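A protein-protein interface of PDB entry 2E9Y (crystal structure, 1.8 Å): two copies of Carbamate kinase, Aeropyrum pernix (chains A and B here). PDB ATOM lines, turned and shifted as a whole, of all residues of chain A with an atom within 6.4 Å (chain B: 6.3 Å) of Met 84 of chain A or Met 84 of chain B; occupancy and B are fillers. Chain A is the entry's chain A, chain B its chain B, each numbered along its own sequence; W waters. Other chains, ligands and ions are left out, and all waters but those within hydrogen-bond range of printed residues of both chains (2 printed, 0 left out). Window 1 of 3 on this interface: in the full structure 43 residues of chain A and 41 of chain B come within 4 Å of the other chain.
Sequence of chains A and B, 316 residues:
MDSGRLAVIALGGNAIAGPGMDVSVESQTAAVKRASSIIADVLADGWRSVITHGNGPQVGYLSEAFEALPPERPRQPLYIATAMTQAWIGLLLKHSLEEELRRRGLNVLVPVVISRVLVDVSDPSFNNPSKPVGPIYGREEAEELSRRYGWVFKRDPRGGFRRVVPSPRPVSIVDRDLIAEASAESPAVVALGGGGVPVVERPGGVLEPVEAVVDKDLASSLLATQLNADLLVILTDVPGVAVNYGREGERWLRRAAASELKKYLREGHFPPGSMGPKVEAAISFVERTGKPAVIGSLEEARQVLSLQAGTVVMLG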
ATOM      1  N   TYR A  61      -1.315 -25.038   2.322  1.00  0.00           N
ATOM      2  CA  TYR A  61      -0.642 -23.794   2.683  1.00  0.00           C
ATOM      3  C   TYR A  61      -1.469 -23.035   3.715  1.00  0.00           C
ATOM      4  O   TYR A  61      -0.944 -22.580   4.736  1.00  0.00           O
ATOM      5  CB  TYR A  61      -0.445 -22.922   1.436  1.00  0.00           C
ATOM      6  CG  TYR A  61      -0.022 -21.493   1.727  1.00  0.00           C
ATOM      7  CD1 TYR A  61       1.287 -21.191   2.099  1.00  0.00           C
ATOM      8  CD2 TYR A  61      -0.936 -20.446   1.628  1.00  0.00           C
ATOM      9  CE1 TYR A  61       1.677 -19.874   2.364  1.00  0.00           C
ATOM     10  CE2 TYR A  61      -0.565 -19.131   1.894  1.00  0.00           C
ATOM     11  CZ  TYR A  61       0.745 -18.849   2.260  1.00  0.00           C
ATOM     12  OH  TYR A  61       1.118 -17.545   2.501  1.00  0.00           O
ATOM     13  N   LEU A  62      -2.766 -22.888   3.452  1.00  0.00           N
ATOM     14  CA  LEU A  62      -3.641 -22.184   4.382  1.00  0.00           C
ATOM     15  C   LEU A  62      -3.678 -22.868   5.744  1.00  0.00           C
ATOM     16  O   LEU A  62      -3.642 -22.207   6.780  1.00  0.00           O
ATOM     17  CB  LEU A  62      -5.055 -22.090   3.811  1.00  0.00           C
ATOM     18  CG  LEU A  62      -5.154 -21.207   2.564  1.00  0.00           C
ATOM     19  CD1 LEU A  62      -6.592 -21.210   2.044  1.00  0.00           C
ATOM     20  CD2 LEU A  62      -4.724 -19.777   2.918  1.00  0.00           C
ATOM     21  N   PHE A  66      -2.584 -20.923   9.294  1.00  0.00           N
ATOM     22  CA  PHE A  66      -3.383 -20.728  10.498  1.00  0.00           C
ATOM     23  C   PHE A  66      -2.749 -21.424  11.702  1.00  0.00           C
ATOM     24  O   PHE A  66      -2.799 -20.912  12.821  1.00  0.00           O
ATOM     25  CB  PHE A  66      -4.819 -21.227  10.273  1.00  0.00           C
ATOM     26  CG  PHE A  66      -5.483 -20.637   9.054  1.00  0.00           C
ATOM     27  CD1 PHE A  66      -5.217 -19.325   8.666  1.00  0.00           C
ATOM     28  CD2 PHE A  66      -6.367 -21.394   8.296  1.00  0.00           C
ATOM     29  CE1 PHE A  66      -5.822 -18.778   7.531  1.00  0.00           C
ATOM     30  CE2 PHE A  66      -6.978 -20.858   7.161  1.00  0.00           C
ATOM     31  CZ  PHE A  66      -6.704 -19.548   6.778  1.00  0.00           C
ATOM     32  N   GLN A  76      -9.059 -21.474  11.372  1.00  0.00           N
ATOM     33  CA  GLN A  76     -10.292 -21.671  10.622  1.00  0.00           C
ATOM     34  C   GLN A  76     -10.410 -23.149  10.277  1.00  0.00           C
ATOM     35  O   GLN A  76      -9.401 -23.827  10.066  1.00  0.00           O
ATOM     36  CB  GLN A  76     -10.275 -20.832   9.341  1.00  0.00           C
ATOM     37  CG  GLN A  76     -10.180 -19.333   9.596  1.00  0.00           C
ATOM     38  CD  GLN A  76     -11.294 -18.834  10.497  1.00  0.00           C
ATOM     39  OE1 GLN A  76     -12.452 -19.229  10.343  1.00  0.00           O
ATOM     40  NE2 GLN A  76     -10.953 -17.958  11.438  1.00  0.00           N
ATOM     41  N   TYR A  79     -13.177 -26.612   5.986  1.00  0.00           N
ATOM     42  CA  TYR A  79     -14.149 -26.240   4.961  1.00  0.00           C
ATOM     43  C   TYR A  79     -14.072 -24.761   4.615  1.00  0.00           C
ATOM     44  O   TYR A  79     -14.386 -24.378   3.489  1.00  0.00           O
ATOM     45  CB  TYR A  79     -15.570 -26.640   5.373  1.00  0.00           C
ATOM     46  CG  TYR A  79     -16.047 -26.086   6.688  1.00  0.00           C
ATOM     47  CD1 TYR A  79     -16.590 -24.810   6.773  1.00  0.00           C
ATOM     48  CD2 TYR A  79     -15.994 -26.864   7.848  1.00  0.00           C
ATOM     49  CE1 TYR A  79     -17.078 -24.315   7.984  1.00  0.00           C
ATOM     50  CE2 TYR A  79     -16.476 -26.383   9.058  1.00  0.00           C
ATOM     51  CZ  TYR A  79     -17.019 -25.109   9.116  1.00  0.00           C
ATOM     52  OH  TYR A  79     -17.510 -24.637  10.312  1.00  0.00           O
ATOM     53  N   ILE A  80     -13.650 -23.935   5.571  1.00  0.00           N
ATOM     54  CA  ILE A  80     -13.489 -22.508   5.308  1.00  0.00           C
ATOM     55  C   ILE A  80     -12.215 -22.344   4.470  1.00  0.00           C
ATOM     56  O   ILE A  80     -12.161 -21.524   3.549  1.00  0.00           O
ATOM     57  CB  ILE A  80     -13.364 -21.695   6.623  1.00  0.00           C
ATOM     58  CG1 ILE A  80     -14.733 -21.606   7.309  1.00  0.00           C
ATOM     59  CG2 ILE A  80     -12.835 -20.292   6.338  1.00  0.00           C
ATOM     60  CD1 ILE A  80     -15.814 -21.009   6.449  1.00  0.00           C
ATOM     61  N   ALA A  81     -11.188 -23.125   4.789  1.00  0.00           N
ATOM     62  CA  ALA A  81      -9.943 -23.072   4.029  1.00  0.00           C
ATOM     63  C   ALA A  81     -10.247 -23.462   2.582  1.00  0.00           C
ATOM     64  O   ALA A  81      -9.780 -22.820   1.639  1.00  0.00           O
ATOM     65  CB  ALA A  81      -8.911 -24.022   4.629  1.00  0.00           C
ATOM     66  N   THR A  82     -11.047 -24.508   2.405  1.00  0.00           N
ATOM     67  CA  THR A  82     -11.407 -24.941   1.060  1.00  0.00           C
ATOM     68  C   THR A  82     -12.150 -23.829   0.316  1.00  0.00           C
ATOM     69  O   THR A  82     -11.859 -23.560  -0.850  1.00  0.00           O
ATOM     70  CB  THR A  82     -12.284 -26.212   1.093  1.00  0.00           C
ATOM     71  OG1 THR A  82     -11.500 -27.312   1.567  1.00  0.00           O
ATOM     72  CG2 THR A  82     -12.815 -26.537  -0.300  1.00  0.00           C
ATOM     73  N   ALA A  83     -13.103 -23.183   0.982  1.00  0.00           N
ATOM     74  CA  ALA A  83     -13.850 -22.091   0.345  1.00  0.00           C
ATOM     75  C   ALA A  83     -12.876 -21.000  -0.090  1.00  0.00           C
ATOM     76  O   ALA A  83     -12.979 -20.448  -1.193  1.00  0.00           O
ATOM     77  CB  ALA A  83     -14.889 -21.517   1.309  1.00  0.00           C
ATOM     78  N   MET A  84     -11.925 -20.683   0.782  1.00  0.00           N
ATOM     79  CA  MET A  84     -10.914 -19.685   0.470  1.00  0.00           C
ATOM     80  C   MET A  84     -10.168 -20.039  -0.814  1.00  0.00           C
ATOM     81  O   MET A  84      -9.911 -19.199  -1.667  1.00  0.00           O
ATOM     82  CB  MET A  84      -9.932 -19.617   1.641  1.00  0.00           C
ATOM     83  CG  MET A  84     -10.487 -18.823   2.825  1.00  0.00           C
ATOM     84  SD  MET A  84      -9.276 -18.621   4.139  1.00  0.00           S
ATOM     85  CE  MET A  84     -10.389 -18.000   5.408  1.00  0.00           C
ATOM     86  N   THR A  85      -9.789 -21.313  -0.960  1.00  0.00           N
ATOM     87  CA  THR A  85      -9.052 -21.718  -2.156  1.00  0.00           C
ATOM     88  C   THR A  85      -9.894 -21.589  -3.423  1.00  0.00           C
ATOM     89  O   THR A  85      -9.349 -21.430  -4.517  1.00  0.00           O
ATOM     90  CB  THR A  85      -8.501 -23.182  -2.068  1.00  0.00           C
ATOM     91  OG1 THR A  85      -9.579 -24.127  -2.037  1.00  0.00           O
ATOM     92  CG2 THR A  85      -7.637 -23.349  -0.829  1.00  0.00           C
ATOM     93  N   GLN A  86     -11.215 -21.667  -3.296  1.00  0.00           N
ATOM     94  CA  GLN A  86     -12.055 -21.527  -4.483  1.00  0.00           C
ATOM     95  C   GLN A  86     -11.955 -20.095  -5.005  1.00  0.00           C
ATOM     96  O   GLN A  86     -11.938 -19.870  -6.213  1.00  0.00           O
ATOM     97  CB  GLN A  86     -13.522 -21.886  -4.185  1.00  0.00           C
ATOM     98  CG  GLN A  86     -13.729 -23.352  -3.797  1.00  0.00           C
ATOM     99  CD  GLN A  86     -15.201 -23.752  -3.676  1.00  0.00           C
ATOM    100  OE1 GLN A  86     -16.083 -22.906  -3.521  1.00  0.00           O
ATOM    101  NE2 GLN A  86     -15.462 -25.058  -3.729  1.00  0.00           N
ATOM    102  N   ALA A  87     -11.873 -19.126  -4.099  1.00  0.00           N
ATOM    103  CA  ALA A  87     -11.757 -17.728  -4.511  1.00  0.00           C
ATOM    104  C   ALA A  87     -10.330 -17.420  -4.968  1.00  0.00           C
ATOM    105  O   ALA A  87     -10.120 -16.693  -5.943  1.00  0.00           O
ATOM    106  CB  ALA A  87     -12.145 -16.810  -3.357  1.00  0.00           C
ATOM    107  N   TRP A  88      -9.355 -17.983  -4.260  1.00  0.00           N
ATOM    108  CA  TRP A  88      -7.944 -17.777  -4.574  1.00  0.00           C
ATOM    109  C   TRP A  88      -7.625 -18.308  -5.978  1.00  0.00           C
ATOM    110  O   TRP A  88      -7.267 -17.539  -6.873  1.00  0.00           O
ATOM    111  CB  TRP A  88      -7.099 -18.472  -3.495  1.00  0.00           C
ATOM    112  CG  TRP A  88      -5.610 -18.563  -3.710  1.00  0.00           C
ATOM    113  CD1 TRP A  88      -4.870 -18.015  -4.726  1.00  0.00           C
ATOM    114  CD2 TRP A  88      -4.684 -19.279  -2.882  1.00  0.00           C
ATOM    115  NE1 TRP A  88      -3.539 -18.357  -4.579  1.00  0.00           N
ATOM    116  CE2 TRP A  88      -3.402 -19.129  -3.453  1.00  0.00           C
ATOM    117  CE3 TRP A  88      -4.819 -20.035  -1.708  1.00  0.00           C
ATOM    118  CZ2 TRP A  88      -2.257 -19.710  -2.888  1.00  0.00           C
ATOM    119  CZ3 TRP A  88      -3.683 -20.612  -1.148  1.00  0.00           C
ATOM    120  CH2 TRP A  88      -2.418 -20.445  -1.741  1.00  0.00           C
ATOM    121  N   ILE A  89      -7.791 -19.610  -6.179  1.00  0.00           N
ATOM    122  CA  ILE A  89      -7.497 -20.213  -7.475  1.00  0.00           C
ATOM    123  C   ILE A  89      -8.499 -19.760  -8.538  1.00  0.00           C
ATOM    124  O   ILE A  89      -8.127 -19.487  -9.687  1.00  0.00           O
ATOM    125  CB  ILE A  89      -7.496 -21.754  -7.368  1.00  0.00           C
ATOM    126  CG1 ILE A  89      -6.440 -22.206  -6.353  1.00  0.00           C
ATOM    127  CG2 ILE A  89      -7.174 -22.374  -8.722  1.00  0.00           C
ATOM    128  CD1 ILE A  89      -6.565 -23.675  -5.944  1.00  0.00           C
ATOM    129  N   TYR B  61      -6.706 -10.984   9.678  1.00  0.00           N
ATOM    130  CA  TYR B  61      -6.387 -12.315  10.195  1.00  0.00           C
ATOM    131  C   TYR B  61      -5.550 -13.094   9.175  1.00  0.00           C
ATOM    132  O   TYR B  61      -4.588 -13.784   9.531  1.00  0.00           O
ATOM    133  CB  TYR B  61      -7.688 -13.075  10.489  1.00  0.00           C
ATOM    134  CG  TYR B  61      -7.515 -14.541  10.843  1.00  0.00           C
ATOM    135  CD1 TYR B  61      -7.246 -14.946  12.158  1.00  0.00           C
ATOM    136  CD2 TYR B  61      -7.652 -15.530   9.868  1.00  0.00           C
ATOM    137  CE1 TYR B  61      -7.126 -16.304  12.486  1.00  0.00           C
ATOM    138  CE2 TYR B  61      -7.531 -16.885  10.185  1.00  0.00           C
ATOM    139  CZ  TYR B  61      -7.274 -17.267  11.493  1.00  0.00           C
ATOM    140  OH  TYR B  61      -7.201 -18.612  11.803  1.00  0.00           O
ATOM    141  N   LEU B  62      -5.919 -12.990   7.905  1.00  0.00           N
ATOM    142  CA  LEU B  62      -5.178 -13.690   6.868  1.00  0.00           C
ATOM    143  C   LEU B  62      -3.744 -13.178   6.784  1.00  0.00           C
ATOM    144  O   LEU B  62      -2.801 -13.965   6.697  1.00  0.00           O
ATOM    145  CB  LEU B  62      -5.869 -13.536   5.512  1.00  0.00           C
ATOM    146  CG  LEU B  62      -7.189 -14.305   5.375  1.00  0.00           C
ATOM    147  CD1 LEU B  62      -7.761 -14.087   3.986  1.00  0.00           C
ATOM    148  CD2 LEU B  62      -6.953 -15.793   5.613  1.00  0.00           C
ATOM    149  N   PHE B  66      -0.360 -15.426   7.294  1.00  0.00           N
ATOM    150  CA  PHE B  66       0.678 -15.555   6.278  1.00  0.00           C
ATOM    151  C   PHE B  66       2.032 -15.136   6.837  1.00  0.00           C
ATOM    152  O   PHE B  66       3.051 -15.772   6.556  1.00  0.00           O
ATOM    153  CB  PHE B  66       0.370 -14.699   5.045  1.00  0.00           C
ATOM    154  CG  PHE B  66      -0.926 -15.041   4.365  1.00  0.00           C
ATOM    155  CD1 PHE B  66      -1.458 -16.324   4.433  1.00  0.00           C
ATOM    156  CD2 PHE B  66      -1.609 -14.072   3.640  1.00  0.00           C
ATOM    157  CE1 PHE B  66      -2.657 -16.634   3.789  1.00  0.00           C
ATOM    158  CE2 PHE B  66      -2.807 -14.374   2.993  1.00  0.00           C
ATOM    159  CZ  PHE B  66      -3.327 -15.656   3.071  1.00  0.00           C
ATOM    160  N   GLN B  76       1.086 -14.468   0.253  1.00  0.00           N
ATOM    161  CA  GLN B  76       0.106 -14.105  -0.761  1.00  0.00           C
ATOM    162  C   GLN B  76      -0.134 -12.603  -0.726  1.00  0.00           C
ATOM    163  O   GLN B  76      -0.106 -11.986   0.340  1.00  0.00           O
ATOM    164  CB  GLN B  76      -1.210 -14.851  -0.522  1.00  0.00           C
ATOM    165  CG  GLN B  76      -1.089 -16.363  -0.653  1.00  0.00           C
ATOM    166  CD  GLN B  76      -0.479 -16.794  -1.974  1.00  0.00           C
ATOM    167  OE1 GLN B  76      -0.944 -16.404  -3.046  1.00  0.00           O
ATOM    168  NE2 GLN B  76       0.568 -17.607  -1.902  1.00  0.00           N
ATOM    169  N   TYR B  79      -4.428  -8.618  -2.604  1.00  0.00           N
ATOM    170  CA  TYR B  79      -5.560  -8.824  -3.497  1.00  0.00           C
ATOM    171  C   TYR B  79      -6.101 -10.252  -3.404  1.00  0.00           C
ATOM    172  O   TYR B  79      -7.309 -10.475  -3.494  1.00  0.00           O
ATOM    173  CB  TYR B  79      -5.172  -8.440  -4.934  1.00  0.00           C
ATOM    174  CG  TYR B  79      -4.621  -9.528  -5.835  1.00  0.00           C
ATOM    175  CD1 TYR B  79      -5.479 -10.396  -6.506  1.00  0.00           C
ATOM    176  CD2 TYR B  79      -3.255  -9.612  -6.107  1.00  0.00           C
ATOM    177  CE1 TYR B  79      -5.004 -11.310  -7.437  1.00  0.00           C
ATOM    178  CE2 TYR B  79      -2.764 -10.528  -7.041  1.00  0.00           C
ATOM    179  CZ  TYR B  79      -3.646 -11.369  -7.705  1.00  0.00           C
ATOM    180  OH  TYR B  79      -3.189 -12.247  -8.664  1.00  0.00           O
ATOM    181  N   ILE B  80      -5.210 -11.212  -3.185  1.00  0.00           N
ATOM    182  CA  ILE B  80      -5.615 -12.605  -3.053  1.00  0.00           C
ATOM    183  C   ILE B  80      -6.271 -12.812  -1.678  1.00  0.00           C
ATOM    184  O   ILE B  80      -7.247 -13.556  -1.552  1.00  0.00           O
ATOM    185  CB  ILE B  80      -4.394 -13.540  -3.252  1.00  0.00           C
ATOM    186  CG1 ILE B  80      -4.031 -13.590  -4.742  1.00  0.00           C
ATOM    187  CG2 ILE B  80      -4.697 -14.940  -2.740  1.00  0.00           C
ATOM    188  CD1 ILE B  80      -5.131 -14.142  -5.624  1.00  0.00           C
ATOM    189  N   ALA B  81      -5.743 -12.149  -0.654  1.00  0.00           N
ATOM    190  CA  ALA B  81      -6.329 -12.251   0.683  1.00  0.00           C
ATOM    191  C   ALA B  81      -7.751 -11.688   0.614  1.00  0.00           C
ATOM    192  O   ALA B  81      -8.691 -12.259   1.168  1.00  0.00           O
ATOM    193  CB  ALA B  81      -5.508 -11.455   1.689  1.00  0.00           C
ATOM    194  N   THR B  82      -7.914 -10.564  -0.075  1.00  0.00           N
ATOM    195  CA  THR B  82      -9.247  -9.978  -0.189  1.00  0.00           C
ATOM    196  C   THR B  82     -10.197 -10.961  -0.867  1.00  0.00           C
ATOM    197  O   THR B  82     -11.325 -11.150  -0.411  1.00  0.00           O
ATOM    198  CB  THR B  82      -9.227  -8.652  -0.981  1.00  0.00           C
ATOM    199  OG1 THR B  82      -8.507  -7.665  -0.232  1.00  0.00           O
ATOM    200  CG2 THR B  82     -10.649  -8.151  -1.212  1.00  0.00           C
ATOM    201  N   ALA B  83      -9.746 -11.582  -1.958  1.00  0.00           N
ATOM    202  CA  ALA B  83     -10.575 -12.557  -2.654  1.00  0.00           C
ATOM    203  C   ALA B  83     -10.936 -13.692  -1.690  1.00  0.00           C
ATOM    204  O   ALA B  83     -12.080 -14.143  -1.651  1.00  0.00           O
ATOM    205  CB  ALA B  83      -9.838 -13.119  -3.860  1.00  0.00           C
ATOM    206  N   MET B  84      -9.957 -14.165  -0.925  1.00  0.00           N
ATOM    207  CA  MET B  84     -10.227 -15.233   0.027  1.00  0.00           C
ATOM    208  C   MET B  84     -11.329 -14.845   1.014  1.00  0.00           C
ATOM    209  O   MET B  84     -12.193 -15.669   1.335  1.00  0.00           O
ATOM    210  CB  MET B  84      -8.955 -15.610   0.785  1.00  0.00           C
ATOM    211  CG  MET B  84      -7.923 -16.318  -0.060  1.00  0.00           C
ATOM    212  SD  MET B  84      -6.468 -16.673   0.968  1.00  0.00           S
ATOM    213  CE  MET B  84      -5.212 -16.993  -0.241  1.00  0.00           C
ATOM    214  N   THR B  85     -11.324 -13.601   1.491  1.00  0.00           N
ATOM    215  CA  THR B  85     -12.370 -13.188   2.433  1.00  0.00           C
ATOM    216  C   THR B  85     -13.743 -13.166   1.776  1.00  0.00           C
ATOM    217  O   THR B  85     -14.757 -13.297   2.459  1.00  0.00           O
ATOM    218  CB  THR B  85     -12.123 -11.784   3.058  1.00  0.00           C
ATOM    219  OG1 THR B  85     -12.165 -10.774   2.038  1.00  0.00           O
ATOM    220  CG2 THR B  85     -10.782 -11.744   3.786  1.00  0.00           C
ATOM    221  N   GLN B  86     -13.792 -12.983   0.458  1.00  0.00           N
ATOM    222  CA  GLN B  86     -15.087 -12.973  -0.221  1.00  0.00           C
ATOM    223  C   GLN B  86     -15.721 -14.359  -0.160  1.00  0.00           C
ATOM    224  O   GLN B  86     -16.934 -14.482   0.035  1.00  0.00           O
ATOM    225  CB  GLN B  86     -14.946 -12.515  -1.679  1.00  0.00           C
ATOM    226  CG  GLN B  86     -14.468 -11.073  -1.801  1.00  0.00           C
ATOM    227  CD  GLN B  86     -14.512 -10.544  -3.229  1.00  0.00           C
ATOM    228  OE1 GLN B  86     -14.543 -11.312  -4.196  1.00  0.00           O
ATOM    229  NE2 GLN B  86     -14.504  -9.222  -3.365  1.00  0.00           N
ATOM    230  N   ALA B  87     -14.904 -15.402  -0.307  1.00  0.00           N
ATOM    231  CA  ALA B  87     -15.412 -16.771  -0.246  1.00  0.00           C
ATOM    232  C   ALA B  87     -15.666 -17.192   1.199  1.00  0.00           C
ATOM    233  O   ALA B  87     -16.616 -17.917   1.488  1.00  0.00           O
ATOM    234  CB  ALA B  87     -14.422 -17.739  -0.907  1.00  0.00           C
ATOM    235  N   TRP B  88     -14.811 -16.728   2.104  1.00  0.00           N
ATOM    236  CA  TRP B  88     -14.927 -17.039   3.530  1.00  0.00           C
ATOM    237  C   TRP B  88     -16.233 -16.492   4.105  1.00  0.00           C
ATOM    238  O   TRP B  88     -17.096 -17.247   4.558  1.00  0.00           O
ATOM    239  CB  TRP B  88     -13.727 -16.431   4.255  1.00  0.00           C
ATOM    240  CG  TRP B  88     -13.693 -16.534   5.757  1.00  0.00           C
ATOM    241  CD1 TRP B  88     -14.600 -17.151   6.580  1.00  0.00           C
ATOM    242  CD2 TRP B  88     -12.701 -15.957   6.615  1.00  0.00           C
ATOM    243  NE1 TRP B  88     -14.230 -16.983   7.895  1.00  0.00           N
ATOM    244  CE2 TRP B  88     -13.069 -16.256   7.943  1.00  0.00           C
ATOM    245  CE3 TRP B  88     -11.531 -15.214   6.385  1.00  0.00           C
ATOM    246  CZ2 TRP B  88     -12.310 -15.834   9.046  1.00  0.00           C
ATOM    247  CZ3 TRP B  88     -10.774 -14.794   7.483  1.00  0.00           C
ATOM    248  CH2 TRP B  88     -11.172 -15.105   8.796  1.00  0.00           C
ATOM    249  N   ILE B  89     -16.373 -15.173   4.076  1.00  0.00           N
ATOM    250  CA  ILE B  89     -17.561 -14.518   4.600  1.00  0.00           C
ATOM    251  C   ILE B  89     -18.766 -14.839   3.720  1.00  0.00           C
ATOM    252  O   ILE B  89     -19.883 -15.033   4.217  1.00  0.00           O
ATOM    253  CB  ILE B  89     -17.349 -12.995   4.652  1.00  0.00           C
ATOM    254  CG1 ILE B  89     -16.164 -12.674   5.570  1.00  0.00           C
ATOM    255  CG2 ILE B  89     -18.620 -12.300   5.135  1.00  0.00           C
ATOM    256  CD1 ILE B  89     -15.632 -11.251   5.428  1.00  0.00           C
HETATM  257  O   HOH W   1       3.552 -17.471   4.381  1.00  0.00           O
HETATM  258  O   HOH W   2     -14.690 -17.812  10.921  1.00  0.00           O
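The backbone NH (N) of Gln 76 of chain A sits at hydrogen-bond distance from the side-chain hydroxyl (OH) of Tyr 61 of chain B, at 3.4 Å.
CD2 of Leu 62 of chain A touches CE1 of Phe 66 of chain B, at 3.9 Å.
CE1 of Phe 66 of chain A touches CD2 of Leu 62 of chain B, at 3.7 Å.
CZ2 of Trp 88 of chain B touches NE2 of Gln 76 of chain A (3.5 Å).
Ala 87 of chain B touches Ala 83 of chain A.
Met 84 of chain A touches Leu 62 of chain B (SD to CD2, 3.9 Å).
O of Ala 83 of chain B touches CB of Ala 87 of chain A, 3.2 Å away.
Ala 87 of chain A touches Ala 87 of chain B.
Trp 88 of chain A touches Gln 76 of chain B.
CD1 of Trp 88 of chain A touches CG2 of Ile 80 of chain B (3.7 Å).
Trp 88 of chain A touches Met 84 of chain B.
Of the printed residues of chain B, Tyr 61 of chain A touches Phe 66 (3.4 Å) and Gln 76 (3.8 Å).
Of the printed residues of chain B, Leu 62 of chain A touches Phe 66 (3.9 Å).
Of the printed residues of chain B, Phe 66 of chain A touches Tyr 61 and Leu 62.
Met 84 of chain A touches just these residues of chain B: Leu 62, Met 84 and Trp 88.
Printed residues of chain B within 4 Å of Ala 87 of chain A: Ala 83 and Ala 87.
Ile 89 of chain A touches none of the printed residues of chain B.
Of the printed residues of chain A, Met 84 of chain B touches Met 84 and Trp 88.
Of the 15 printed residues of chain A, 9 touch a printed residue of chain B.
Hydrophobic or aromatic side chains of chain A that line the printed part of chain B: Tyr 61, Leu 62, Phe 66, Ile 80, Ala 83, Met 84, Ala 87 and Trp 88.
Hydrophobic or aromatic side chains of chain B within 4 Å of the printed part of chain A: Tyr 61, Leu 62, Phe 66, Ile 80, Met 84, Ala 87 and Trp 88.
Among the printed residues, 17 pairs touch across the chains.
Tyr 61 of chain A touches Gln 76 of chain B, and with the chains exchanged Gln 76 of chain A touches Tyr 61 of chain B.
Leu 62 of chain A touches Phe 66 of chain B, and with the chains exchanged Phe 66 of chain A touches Leu 62 of chain B.
Gln 76 of chain A touches Trp 88 of chain B, and with the chains exchanged Trp 88 of chain A touches Gln 76 of chain B.
Ala 87 of chain A touches its own counterpart, Ala 87 of chain B.
Of the 17 pairs that touch across the chains among the printed residues, 16 have their exchanged pair printed and touching as well.
Water W2 bridges OE1 of Gln 76 of chain A (2.7 Å) and NE1 of Trp 88 of chain B (3.2 Å).
Water W1 lies within hydrogen-bond range of the backbone carbonyl oxygen (O) of Phe 66 of chain B (2.8 Å) and the side-chain hydroxyl (OH) of Tyr 61 of chain A (3.1 Å).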
